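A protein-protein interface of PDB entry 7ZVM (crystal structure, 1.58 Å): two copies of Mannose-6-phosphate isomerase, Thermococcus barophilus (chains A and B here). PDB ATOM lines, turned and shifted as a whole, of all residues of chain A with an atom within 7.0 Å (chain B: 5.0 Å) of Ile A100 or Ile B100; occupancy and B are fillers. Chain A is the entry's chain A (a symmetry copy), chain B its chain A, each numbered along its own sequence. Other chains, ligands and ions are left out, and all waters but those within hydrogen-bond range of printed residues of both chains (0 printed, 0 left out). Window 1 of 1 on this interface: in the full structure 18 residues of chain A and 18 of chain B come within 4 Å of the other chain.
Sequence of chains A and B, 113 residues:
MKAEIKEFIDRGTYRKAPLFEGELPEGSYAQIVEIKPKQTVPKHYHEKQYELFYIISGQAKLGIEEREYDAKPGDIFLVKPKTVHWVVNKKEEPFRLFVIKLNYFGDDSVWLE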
ATOM      1  N   LEU A  24      17.697  29.137 -12.999  1.00  0.00           N
ATOM      2  CA  LEU A  24      19.136  28.900 -13.291  1.00  0.00           C
ATOM      3  C   LEU A  24      19.997  29.695 -12.321  1.00  0.00           C
ATOM      4  O   LEU A  24      19.552  30.745 -11.824  1.00  0.00           O
ATOM      5  CB  LEU A  24      19.454  29.300 -14.722  1.00  0.00           C
ATOM      6  CG  LEU A  24      18.722  28.527 -15.819  1.00  0.00           C
ATOM      7  CD1 LEU A  24      19.258  28.879 -17.217  1.00  0.00           C
ATOM      8  CD2 LEU A  24      18.798  27.050 -15.617  1.00  0.00           C
ATOM      9  N   SER A  28      23.811  32.653 -15.485  1.00  0.00           N
ATOM     10  CA  SER A  28      23.435  31.731 -16.571  1.00  0.00           C
ATOM     11  C   SER A  28      22.016  32.087 -16.986  1.00  0.00           C
ATOM     12  O   SER A  28      21.249  32.651 -16.167  1.00  0.00           O
ATOM     13  CB  SER A  28      23.620  30.277 -16.165  1.00  0.00           C
ATOM     14  OG  SER A  28      22.607  29.913 -15.262  1.00  0.00           O
ATOM     15  N   TYR A  29      21.699  31.812 -18.236  1.00  0.00           N
ATOM     16  CA  TYR A  29      20.374  32.099 -18.798  1.00  0.00           C
ATOM     17  C   TYR A  29      20.157  31.141 -19.961  1.00  0.00           C
ATOM     18  O   TYR A  29      21.122  30.771 -20.636  1.00  0.00           O
ATOM     19  CB  TYR A  29      20.333  33.550 -19.261  1.00  0.00           C
ATOM     20  CG  TYR A  29      18.975  34.038 -19.648  1.00  0.00           C
ATOM     21  CD1 TYR A  29      18.566  33.997 -20.967  1.00  0.00           C
ATOM     22  CD2 TYR A  29      18.116  34.564 -18.703  1.00  0.00           C
ATOM     23  CE1 TYR A  29      17.314  34.444 -21.326  1.00  0.00           C
ATOM     24  CE2 TYR A  29      16.863  35.005 -19.046  1.00  0.00           C
ATOM     25  CZ  TYR A  29      16.474  34.977 -20.374  1.00  0.00           C
ATOM     26  OH  TYR A  29      15.210  35.414 -20.699  1.00  0.00           O
ATOM     27  N   ALA A  30      18.920  30.756 -20.173  1.00  0.00           N
ATOM     28  CA  ALA A  30      18.597  29.845 -21.285  1.00  0.00           C
ATOM     29  C   ALA A  30      17.352  30.326 -22.012  1.00  0.00           C
ATOM     30  O   ALA A  30      16.454  30.843 -21.396  1.00  0.00           O
ATOM     31  CB  ALA A  30      18.452  28.425 -20.842  1.00  0.00           C
ATOM     32  N   GLN A  31      17.346  30.125 -23.310  1.00  0.00           N
ATOM     33  CA  GLN A  31      16.184  30.539 -24.102  1.00  0.00           C
ATOM     34  C   GLN A  31      16.175  29.802 -25.430  1.00  0.00           C
ATOM     35  O   GLN A  31      17.193  29.249 -25.865  1.00  0.00           O
ATOM     36  CB  GLN A  31      16.158  32.062 -24.301  1.00  0.00           C
ATOM     37  CG  GLN A  31      17.347  32.537 -25.076  1.00  0.00           C
ATOM     38  CD  GLN A  31      17.420  34.035 -25.154  1.00  0.00           C
ATOM     39  OE1 GLN A  31      16.582  34.757 -24.631  1.00  0.00           O
ATOM     40  NE2 GLN A  31      18.410  34.509 -25.878  1.00  0.00           N
ATOM     41  N   GLN A  49      29.609  37.912 -21.754  1.00  0.00           N
ATOM     42  CA  GLN A  49      28.899  36.618 -21.827  1.00  0.00           C
ATOM     43  C   GLN A  49      29.478  35.735 -22.918  1.00  0.00           C
ATOM     44  O   GLN A  49      29.941  36.219 -23.934  1.00  0.00           O
ATOM     45  CB  GLN A  49      27.390  36.705 -22.005  1.00  0.00           C
ATOM     46  CG  GLN A  49      26.925  37.180 -23.360  1.00  0.00           C
ATOM     47  CD  GLN A  49      25.420  37.279 -23.515  1.00  0.00           C
ATOM     48  OE1 GLN A  49      24.743  36.302 -23.775  1.00  0.00           O
ATOM     49  NE2 GLN A  49      24.873  38.483 -23.468  1.00  0.00           N
ATOM     50  N   TYR A  50      29.369  34.441 -22.662  1.00  0.00           N
ATOM     51  CA  TYR A  50      29.599  33.364 -23.646  1.00  0.00           C
ATOM     52  C   TYR A  50      28.226  32.868 -24.105  1.00  0.00           C
ATOM     53  O   TYR A  50      27.257  32.852 -23.239  1.00  0.00           O
ATOM     54  CB  TYR A  50      30.303  32.170 -23.029  1.00  0.00           C
ATOM     55  CG  TYR A  50      31.701  32.402 -22.559  1.00  0.00           C
ATOM     56  CD1 TYR A  50      31.930  33.242 -21.481  1.00  0.00           C
ATOM     57  CD2 TYR A  50      32.774  31.776 -23.176  1.00  0.00           C
ATOM     58  CE1 TYR A  50      33.203  33.401 -20.983  1.00  0.00           C
ATOM     59  CE2 TYR A  50      34.064  31.931 -22.701  1.00  0.00           C
ATOM     60  CZ  TYR A  50      34.264  32.772 -21.625  1.00  0.00           C
ATOM     61  OH  TYR A  50      35.513  32.982 -21.175  1.00  0.00           O
ATOM     62  N   GLU A  51      28.112  32.444 -25.355  1.00  0.00           N
ATOM     63  CA  GLU A  51      26.830  31.874 -25.831  1.00  0.00           C
ATOM     64  C   GLU A  51      27.095  30.525 -26.467  1.00  0.00           C
ATOM     65  O   GLU A  51      27.947  30.410 -27.274  1.00  0.00           O
ATOM     66  CB  GLU A  51      26.188  32.779 -26.845  1.00  0.00           C
ATOM     67  CG  GLU A  51      25.692  34.039 -26.193  1.00  0.00           C
ATOM     68  CD  GLU A  51      24.708  34.740 -27.107  1.00  0.00           C
ATOM     69  OE1 GLU A  51      25.135  35.115 -28.243  1.00  0.00           O
ATOM     70  OE2 GLU A  51      23.536  34.847 -26.721  1.00  0.00           O
ATOM     71  N   LEU A  52      26.382  29.539 -25.984  1.00  0.00           N
ATOM     72  CA  LEU A  52      26.331  28.209 -26.593  1.00  0.00           C
ATOM     73  C   LEU A  52      25.018  28.106 -27.342  1.00  0.00           C
ATOM     74  O   LEU A  52      23.970  28.445 -26.746  1.00  0.00           O
ATOM     75  CB  LEU A  52      26.277  27.174 -25.476  1.00  0.00           C
ATOM     76  CG  LEU A  52      27.540  26.584 -24.956  1.00  0.00           C
ATOM     77  CD1 LEU A  52      27.189  25.633 -23.793  1.00  0.00           C
ATOM     78  CD2 LEU A  52      28.290  25.823 -26.015  1.00  0.00           C
ATOM     79  N   PHE A  53      25.078  27.638 -28.565  1.00  0.00           N
ATOM     80  CA  PHE A  53      23.902  27.548 -29.477  1.00  0.00           C
ATOM     81  C   PHE A  53      23.832  26.094 -29.943  1.00  0.00           C
ATOM     82  O   PHE A  53      24.815  25.565 -30.370  1.00  0.00           O
ATOM     83  CB  PHE A  53      24.092  28.342 -30.782  1.00  0.00           C
ATOM     84  CG  PHE A  53      24.388  29.799 -30.711  1.00  0.00           C
ATOM     85  CD1 PHE A  53      23.779  30.578 -29.748  1.00  0.00           C
ATOM     86  CD2 PHE A  53      25.062  30.435 -31.753  1.00  0.00           C
ATOM     87  CE1 PHE A  53      23.894  31.960 -29.740  1.00  0.00           C
ATOM     88  CE2 PHE A  53      25.171  31.814 -31.741  1.00  0.00           C
ATOM     89  CZ  PHE A  53      24.627  32.570 -30.708  1.00  0.00           C
ATOM     90  N   TYR A  54      22.668  25.489 -29.844  1.00  0.00           N
ATOM     91  CA  TYR A  54      22.289  24.204 -30.438  1.00  0.00           C
ATOM     92  C   TYR A  54      21.258  24.520 -31.513  1.00  0.00           C
ATOM     93  O   TYR A  54      20.247  25.146 -31.192  1.00  0.00           O
ATOM     94  CB  TYR A  54      21.693  23.258 -29.398  1.00  0.00           C
ATOM     95  CG  TYR A  54      21.353  21.937 -30.019  1.00  0.00           C
ATOM     96  CD1 TYR A  54      20.120  21.700 -30.597  1.00  0.00           C
ATOM     97  CD2 TYR A  54      22.283  20.925 -30.023  1.00  0.00           C
ATOM     98  CE1 TYR A  54      19.853  20.505 -31.236  1.00  0.00           C
ATOM     99  CE2 TYR A  54      22.025  19.716 -30.622  1.00  0.00           C
ATOM    100  CZ  TYR A  54      20.824  19.516 -31.243  1.00  0.00           C
ATOM    101  OH  TYR A  54      20.656  18.315 -31.854  1.00  0.00           O
ATOM    102  N   LEU A  78      29.931  27.817 -30.137  1.00  0.00           N
ATOM    103  CA  LEU A  78      30.283  28.628 -28.955  1.00  0.00           C
ATOM    104  C   LEU A  78      30.717  30.018 -29.437  1.00  0.00           C
ATOM    105  O   LEU A  78      31.610  30.114 -30.310  1.00  0.00           O
ATOM    106  CB  LEU A  78      31.436  27.978 -28.199  1.00  0.00           C
ATOM    107  CG  LEU A  78      31.926  28.803 -27.015  1.00  0.00           C
ATOM    108  CD1 LEU A  78      30.848  28.963 -25.939  1.00  0.00           C
ATOM    109  CD2 LEU A  78      33.147  28.134 -26.451  1.00  0.00           C
ATOM    110  N   PHE A  98      18.547  26.683 -29.539  1.00  0.00           N
ATOM    111  CA  PHE A  98      18.544  26.606 -28.083  1.00  0.00           C
ATOM    112  C   PHE A  98      19.822  27.322 -27.677  1.00  0.00           C
ATOM    113  O   PHE A  98      20.918  26.890 -28.162  1.00  0.00           O
ATOM    114  CB  PHE A  98      18.547  25.150 -27.641  1.00  0.00           C
ATOM    115  CG  PHE A  98      18.783  24.886 -26.188  1.00  0.00           C
ATOM    116  CD1 PHE A  98      18.288  25.691 -25.189  1.00  0.00           C
ATOM    117  CD2 PHE A  98      19.573  23.801 -25.855  1.00  0.00           C
ATOM    118  CE1 PHE A  98      18.535  25.380 -23.859  1.00  0.00           C
ATOM    119  CE2 PHE A  98      19.778  23.475 -24.530  1.00  0.00           C
ATOM    120  CZ  PHE A  98      19.306  24.295 -23.535  1.00  0.00           C
ATOM    121  N   VAL A  99      19.664  28.360 -26.861  1.00  0.00           N
ATOM    122  CA  VAL A  99      20.765  29.283 -26.477  1.00  0.00           C
ATOM    123  C   VAL A  99      20.985  29.188 -24.972  1.00  0.00           C
ATOM    124  O   VAL A  99      20.022  29.372 -24.216  1.00  0.00           O
ATOM    125  CB  VAL A  99      20.479  30.741 -26.907  1.00  0.00           C
ATOM    126  CG1 VAL A  99      21.635  31.598 -26.506  1.00  0.00           C
ATOM    127  CG2 VAL A  99      20.262  30.815 -28.399  1.00  0.00           C
ATOM    128  N   ILE A 100      22.229  28.950 -24.588  1.00  0.00           N
ATOM    129  CA  ILE A 100      22.650  29.048 -23.160  1.00  0.00           C
ATOM    130  C   ILE A 100      23.670  30.165 -23.045  1.00  0.00           C
ATOM    131  O   ILE A 100      24.663  30.142 -23.740  1.00  0.00           O
ATOM    132  CB  ILE A 100      23.182  27.702 -22.612  1.00  0.00           C
ATOM    133  CG1 ILE A 100      22.254  26.532 -22.948  1.00  0.00           C
ATOM    134  CG2 ILE A 100      23.378  27.843 -21.131  1.00  0.00           C
ATOM    135  CD1 ILE A 100      22.574  25.866 -24.309  1.00  0.00           C
ATOM    136  N   LYS A 101      23.385  31.130 -22.188  1.00  0.00           N
ATOM    137  CA  LYS A 101      24.323  32.226 -21.924  1.00  0.00           C
ATOM    138  C   LYS A 101      25.055  31.924 -20.620  1.00  0.00           C
ATOM    139  O   LYS A 101      24.418  31.577 -19.648  1.00  0.00           O
ATOM    140  CB  LYS A 101      23.527  33.520 -21.785  1.00  0.00           C
ATOM    141  CG  LYS A 101      22.717  33.902 -23.021  1.00  0.00           C
ATOM    142  CD  LYS A 101      21.908  35.162 -22.706  1.00  0.00           C
ATOM    143  CE  LYS A 101      21.137  35.735 -23.869  1.00  0.00           C
ATOM    144  NZ  LYS A 101      22.035  36.067 -25.014  1.00  0.00           N
ATOM    145  N   LEU A 102      26.354  32.120 -20.636  1.00  0.00           N
ATOM    146  CA  LEU A 102      27.225  31.868 -19.489  1.00  0.00           C
ATOM    147  C   LEU A 102      28.023  33.133 -19.193  1.00  0.00           C
ATOM    148  O   LEU A 102      28.320  33.898 -20.126  1.00  0.00           O
ATOM    149  CB  LEU A 102      28.143  30.725 -19.895  1.00  0.00           C
ATOM    150  CG  LEU A 102      27.467  29.426 -20.316  1.00  0.00           C
ATOM    151  CD1 LEU A 102      28.527  28.477 -20.788  1.00  0.00           C
ATOM    152  CD2 LEU A 102      26.666  28.792 -19.188  1.00  0.00           C
ATOM    153  N   TYR B  29      30.263  23.477 -18.057  1.00  0.00           N
ATOM    154  CA  TYR B  29      30.785  22.337 -18.819  1.00  0.00           C
ATOM    155  C   TYR B  29      29.700  21.912 -19.800  1.00  0.00           C
ATOM    156  O   TYR B  29      28.512  22.045 -19.492  1.00  0.00           O
ATOM    157  CB  TYR B  29      31.130  21.209 -17.854  1.00  0.00           C
ATOM    158  CG  TYR B  29      31.879  20.073 -18.472  1.00  0.00           C
ATOM    159  CD1 TYR B  29      31.203  18.962 -18.940  1.00  0.00           C
ATOM    160  CD2 TYR B  29      33.256  20.099 -18.562  1.00  0.00           C
ATOM    161  CE1 TYR B  29      31.891  17.914 -19.512  1.00  0.00           C
ATOM    162  CE2 TYR B  29      33.952  19.066 -19.137  1.00  0.00           C
ATOM    163  CZ  TYR B  29      33.265  17.950 -19.582  1.00  0.00           C
ATOM    164  OH  TYR B  29      33.978  16.927 -20.165  1.00  0.00           O
ATOM    165  N   ALA B  30      30.114  21.422 -20.945  1.00  0.00           N
ATOM    166  CA  ALA B  30      29.147  20.962 -21.958  1.00  0.00           C
ATOM    167  C   ALA B  30      29.595  19.634 -22.545  1.00  0.00           C
ATOM    168  O   ALA B  30      30.768  19.409 -22.708  1.00  0.00           O
ATOM    169  CB  ALA B  30      28.910  21.977 -23.030  1.00  0.00           C
ATOM    170  N   TYR B  50      23.902  22.239 -11.475  1.00  0.00           N
ATOM    171  CA  TYR B  50      22.624  22.203 -12.216  1.00  0.00           C
ATOM    172  C   TYR B  50      22.901  21.534 -13.564  1.00  0.00           C
ATOM    173  O   TYR B  50      24.052  21.744 -14.130  1.00  0.00           O
ATOM    174  CB  TYR B  50      22.107  23.596 -12.526  1.00  0.00           C
ATOM    175  CG  TYR B  50      21.707  24.425 -11.350  1.00  0.00           C
ATOM    176  CD1 TYR B  50      22.675  24.857 -10.457  1.00  0.00           C
ATOM    177  CD2 TYR B  50      20.383  24.784 -11.147  1.00  0.00           C
ATOM    178  CE1 TYR B  50      22.336  25.690  -9.415  1.00  0.00           C
ATOM    179  CE2 TYR B  50      20.017  25.610 -10.100  1.00  0.00           C
ATOM    180  CZ  TYR B  50      21.001  26.027  -9.226  1.00  0.00           C
ATOM    181  OH  TYR B  50      20.665  26.788  -8.171  1.00  0.00           O
ATOM    182  N   GLU B  51      21.932  20.807 -14.099  1.00  0.00           N
ATOM    183  CA  GLU B  51      22.111  20.204 -15.441  1.00  0.00           C
ATOM    184  C   GLU B  51      20.931  20.581 -16.313  1.00  0.00           C
ATOM    185  O   GLU B  51      19.831  20.432 -15.914  1.00  0.00           O
ATOM    186  CB  GLU B  51      22.195  18.707 -15.346  1.00  0.00           C
ATOM    187  CG  GLU B  51      23.483  18.287 -14.694  1.00  0.00           C
ATOM    188  CD  GLU B  51      23.746  16.821 -14.966  1.00  0.00           C
ATOM    189  OE1 GLU B  51      22.887  15.987 -14.543  1.00  0.00           O
ATOM    190  OE2 GLU B  51      24.744  16.529 -15.640  1.00  0.00           O
ATOM    191  N   LEU B  52      21.245  21.143 -17.453  1.00  0.00           N
ATOM    192  CA  LEU B  52      20.278  21.390 -18.522  1.00  0.00           C
ATOM    193  C   LEU B  52      20.493  20.328 -19.581  1.00  0.00           C
ATOM    194  O   LEU B  52      21.663  20.118 -19.976  1.00  0.00           O
ATOM    195  CB  LEU B  52      20.615  22.727 -19.173  1.00  0.00           C
ATOM    196  CG  LEU B  52      19.967  23.972 -18.677  1.00  0.00           C
ATOM    197  CD1 LEU B  52      20.549  25.167 -19.462  1.00  0.00           C
ATOM    198  CD2 LEU B  52      18.473  23.942 -18.845  1.00  0.00           C
ATOM    199  N   PHE B  98      22.175  16.660 -25.277  1.00  0.00           N
ATOM    200  CA  PHE B  98      23.133  17.753 -25.159  1.00  0.00           C
ATOM    201  C   PHE B  98      22.973  18.224 -23.722  1.00  0.00           C
ATOM    202  O   PHE B  98      21.810  18.586 -23.347  1.00  0.00           O
ATOM    203  CB  PHE B  98      22.793  18.851 -26.156  1.00  0.00           C
ATOM    204  CG  PHE B  98      23.527  20.146 -26.010  1.00  0.00           C
ATOM    205  CD1 PHE B  98      24.851  20.222 -25.644  1.00  0.00           C
ATOM    206  CD2 PHE B  98      22.814  21.312 -26.217  1.00  0.00           C
ATOM    207  CE1 PHE B  98      25.474  21.457 -25.540  1.00  0.00           C
ATOM    208  CE2 PHE B  98      23.452  22.535 -26.153  1.00  0.00           C
ATOM    209  CZ  PHE B  98      24.766  22.609 -25.761  1.00  0.00           C
ATOM    210  N   VAL B  99      24.077  18.192 -22.980  1.00  0.00           N
ATOM    211  CA  VAL B  99      24.096  18.459 -21.518  1.00  0.00           C
ATOM    212  C   VAL B  99      24.950  19.695 -21.255  1.00  0.00           C
ATOM    213  O   VAL B  99      26.109  19.721 -21.685  1.00  0.00           O
ATOM    214  CB  VAL B  99      24.611  17.245 -20.711  1.00  0.00           C
ATOM    215  CG1 VAL B  99      24.581  17.585 -19.256  1.00  0.00           C
ATOM    216  CG2 VAL B  99      23.756  16.031 -20.985  1.00  0.00           C
ATOM    217  N   ILE B 100      24.375  20.645 -20.535  1.00  0.00           N
ATOM    218  CA  ILE B 100      25.142  21.810 -20.004  1.00  0.00           C
ATOM    219  C   ILE B 100      25.112  21.744 -18.489  1.00  0.00           C
ATOM    220  O   ILE B 100      24.045  21.689 -17.915  1.00  0.00           O
ATOM    221  CB  ILE B 100      24.612  23.157 -20.549  1.00  0.00           C
ATOM    222  CG1 ILE B 100      24.415  23.132 -22.067  1.00  0.00           C
ATOM    223  CG2 ILE B 100      25.567  24.240 -20.135  1.00  0.00           C
ATOM    224  CD1 ILE B 100      23.009  22.645 -22.496  1.00  0.00           C
ATOM    225  N   LYS B 101      26.286  21.724 -17.882  1.00  0.00           N
ATOM    226  CA  LYS B 101      26.395  21.741 -16.419  1.00  0.00           C
ATOM    227  C   LYS B 101      26.720  23.166 -15.982  1.00  0.00           C
ATOM    228  O   LYS B 101      27.603  23.775 -16.548  1.00  0.00           O
ATOM    229  CB  LYS B 101      27.524  20.802 -16.008  1.00  0.00           C
ATOM    230  CG  LYS B 101      27.327  19.349 -16.433  1.00  0.00           C
ATOM    231  CD  LYS B 101      28.569  18.550 -16.034  1.00  0.00           C
ATOM    232  CE  LYS B 101      28.482  17.064 -16.286  1.00  0.00           C
ATOM    233  NZ  LYS B 101      27.322  16.453 -15.572  1.00  0.00           N
ATOM    234  N   LEU B 102      26.032  23.619 -14.959  1.00  0.00           N
ATOM    235  CA  LEU B 102      26.190  24.966 -14.410  1.00  0.00           C
ATOM    236  C   LEU B 102      26.477  24.855 -12.917  1.00  0.00           C
ATOM    237  O   LEU B 102      26.004  23.902 -12.274  1.00  0.00           O
ATOM    238  CB  LEU B 102      24.873  25.685 -14.660  1.00  0.00           C
ATOM    239  CG  LEU B 102      24.414  25.777 -16.110  1.00  0.00           C
ATOM    240  CD1 LEU B 102      23.055  26.408 -16.133  1.00  0.00           C
ATOM    241  CD2 LEU B 102      25.374  26.580 -16.977  1.00  0.00           C
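O of Leu B102 sits at hydrogen-bond distance from N of Tyr B50 (2.8 Å). The backbone carbonyl oxygen of Phe A98 sits at hydrogen-bond distance from the backbone NH of Tyr A54. N of Ile B100 lies within hydrogen-bond range of O of Leu B52 (2.8 Å). The backbone carbonyl oxygen of Leu A52 sits at hydrogen-bond distance from the backbone NH of Ile A100 (2.8 Å). The backbone NH of Tyr A50 is in hydrogen-bond range of the backbone carbonyl oxygen of Leu A102.
Among the printed residues, merely in contact across the chains: Leu A102 with Leu B102, Ser A28 with Leu B102, Ile A100 with Ile B100, Tyr A54 with Phe B98, Phe A98 with Ile B100 and Ile A100 with Phe B98.
Of the printed residues of chain B, Ser A28 touches Leu B102 (3.6 Å). Gln A31 touches none of the printed residues of chain B. Ile A100 touches just these residues of chain B: Phe B98 (3.9 Å) and Ile B100 (3.7 Å). Of the printed residues of chain B, Leu A102 touches Leu B102 (3.4 Å). Of the printed residues of chain A, Phe B98 touches Tyr A54 (3.8 Å) and Ile A100 (3.9 Å). Of chain A, only Phe A98 and Ile A100 come within 4 Å of Ile B100. Lys B101 touches none of the printed residues of chain A. The nearest residue of chain B that does not touch Ile A100 is Leu B52 (4.1 Å). The nearest printed residue of chain A that does not touch Leu B102 is Leu A24 (4.3 Å).
Hydrophobic or aromatic side chains of chain A within 4 Å of the printed part of chain B: Tyr A54, Phe A98, Ile A100 and Leu A102.
Phe A98 touches Ile B100, and with the chains exchanged Ile A100 touches Phe B98. Ile B100 touches its own counterpart, Ile A100. Leu A102 touches its own counterpart, Leu B102. Positions printed for both chains: 29, 30, 50, 51, 52, 98, 99, 100, 101 and 102. Of the 6 pairs that touch across the chains among the printed residues, 4 have their exchanged pair printed and touching as well.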
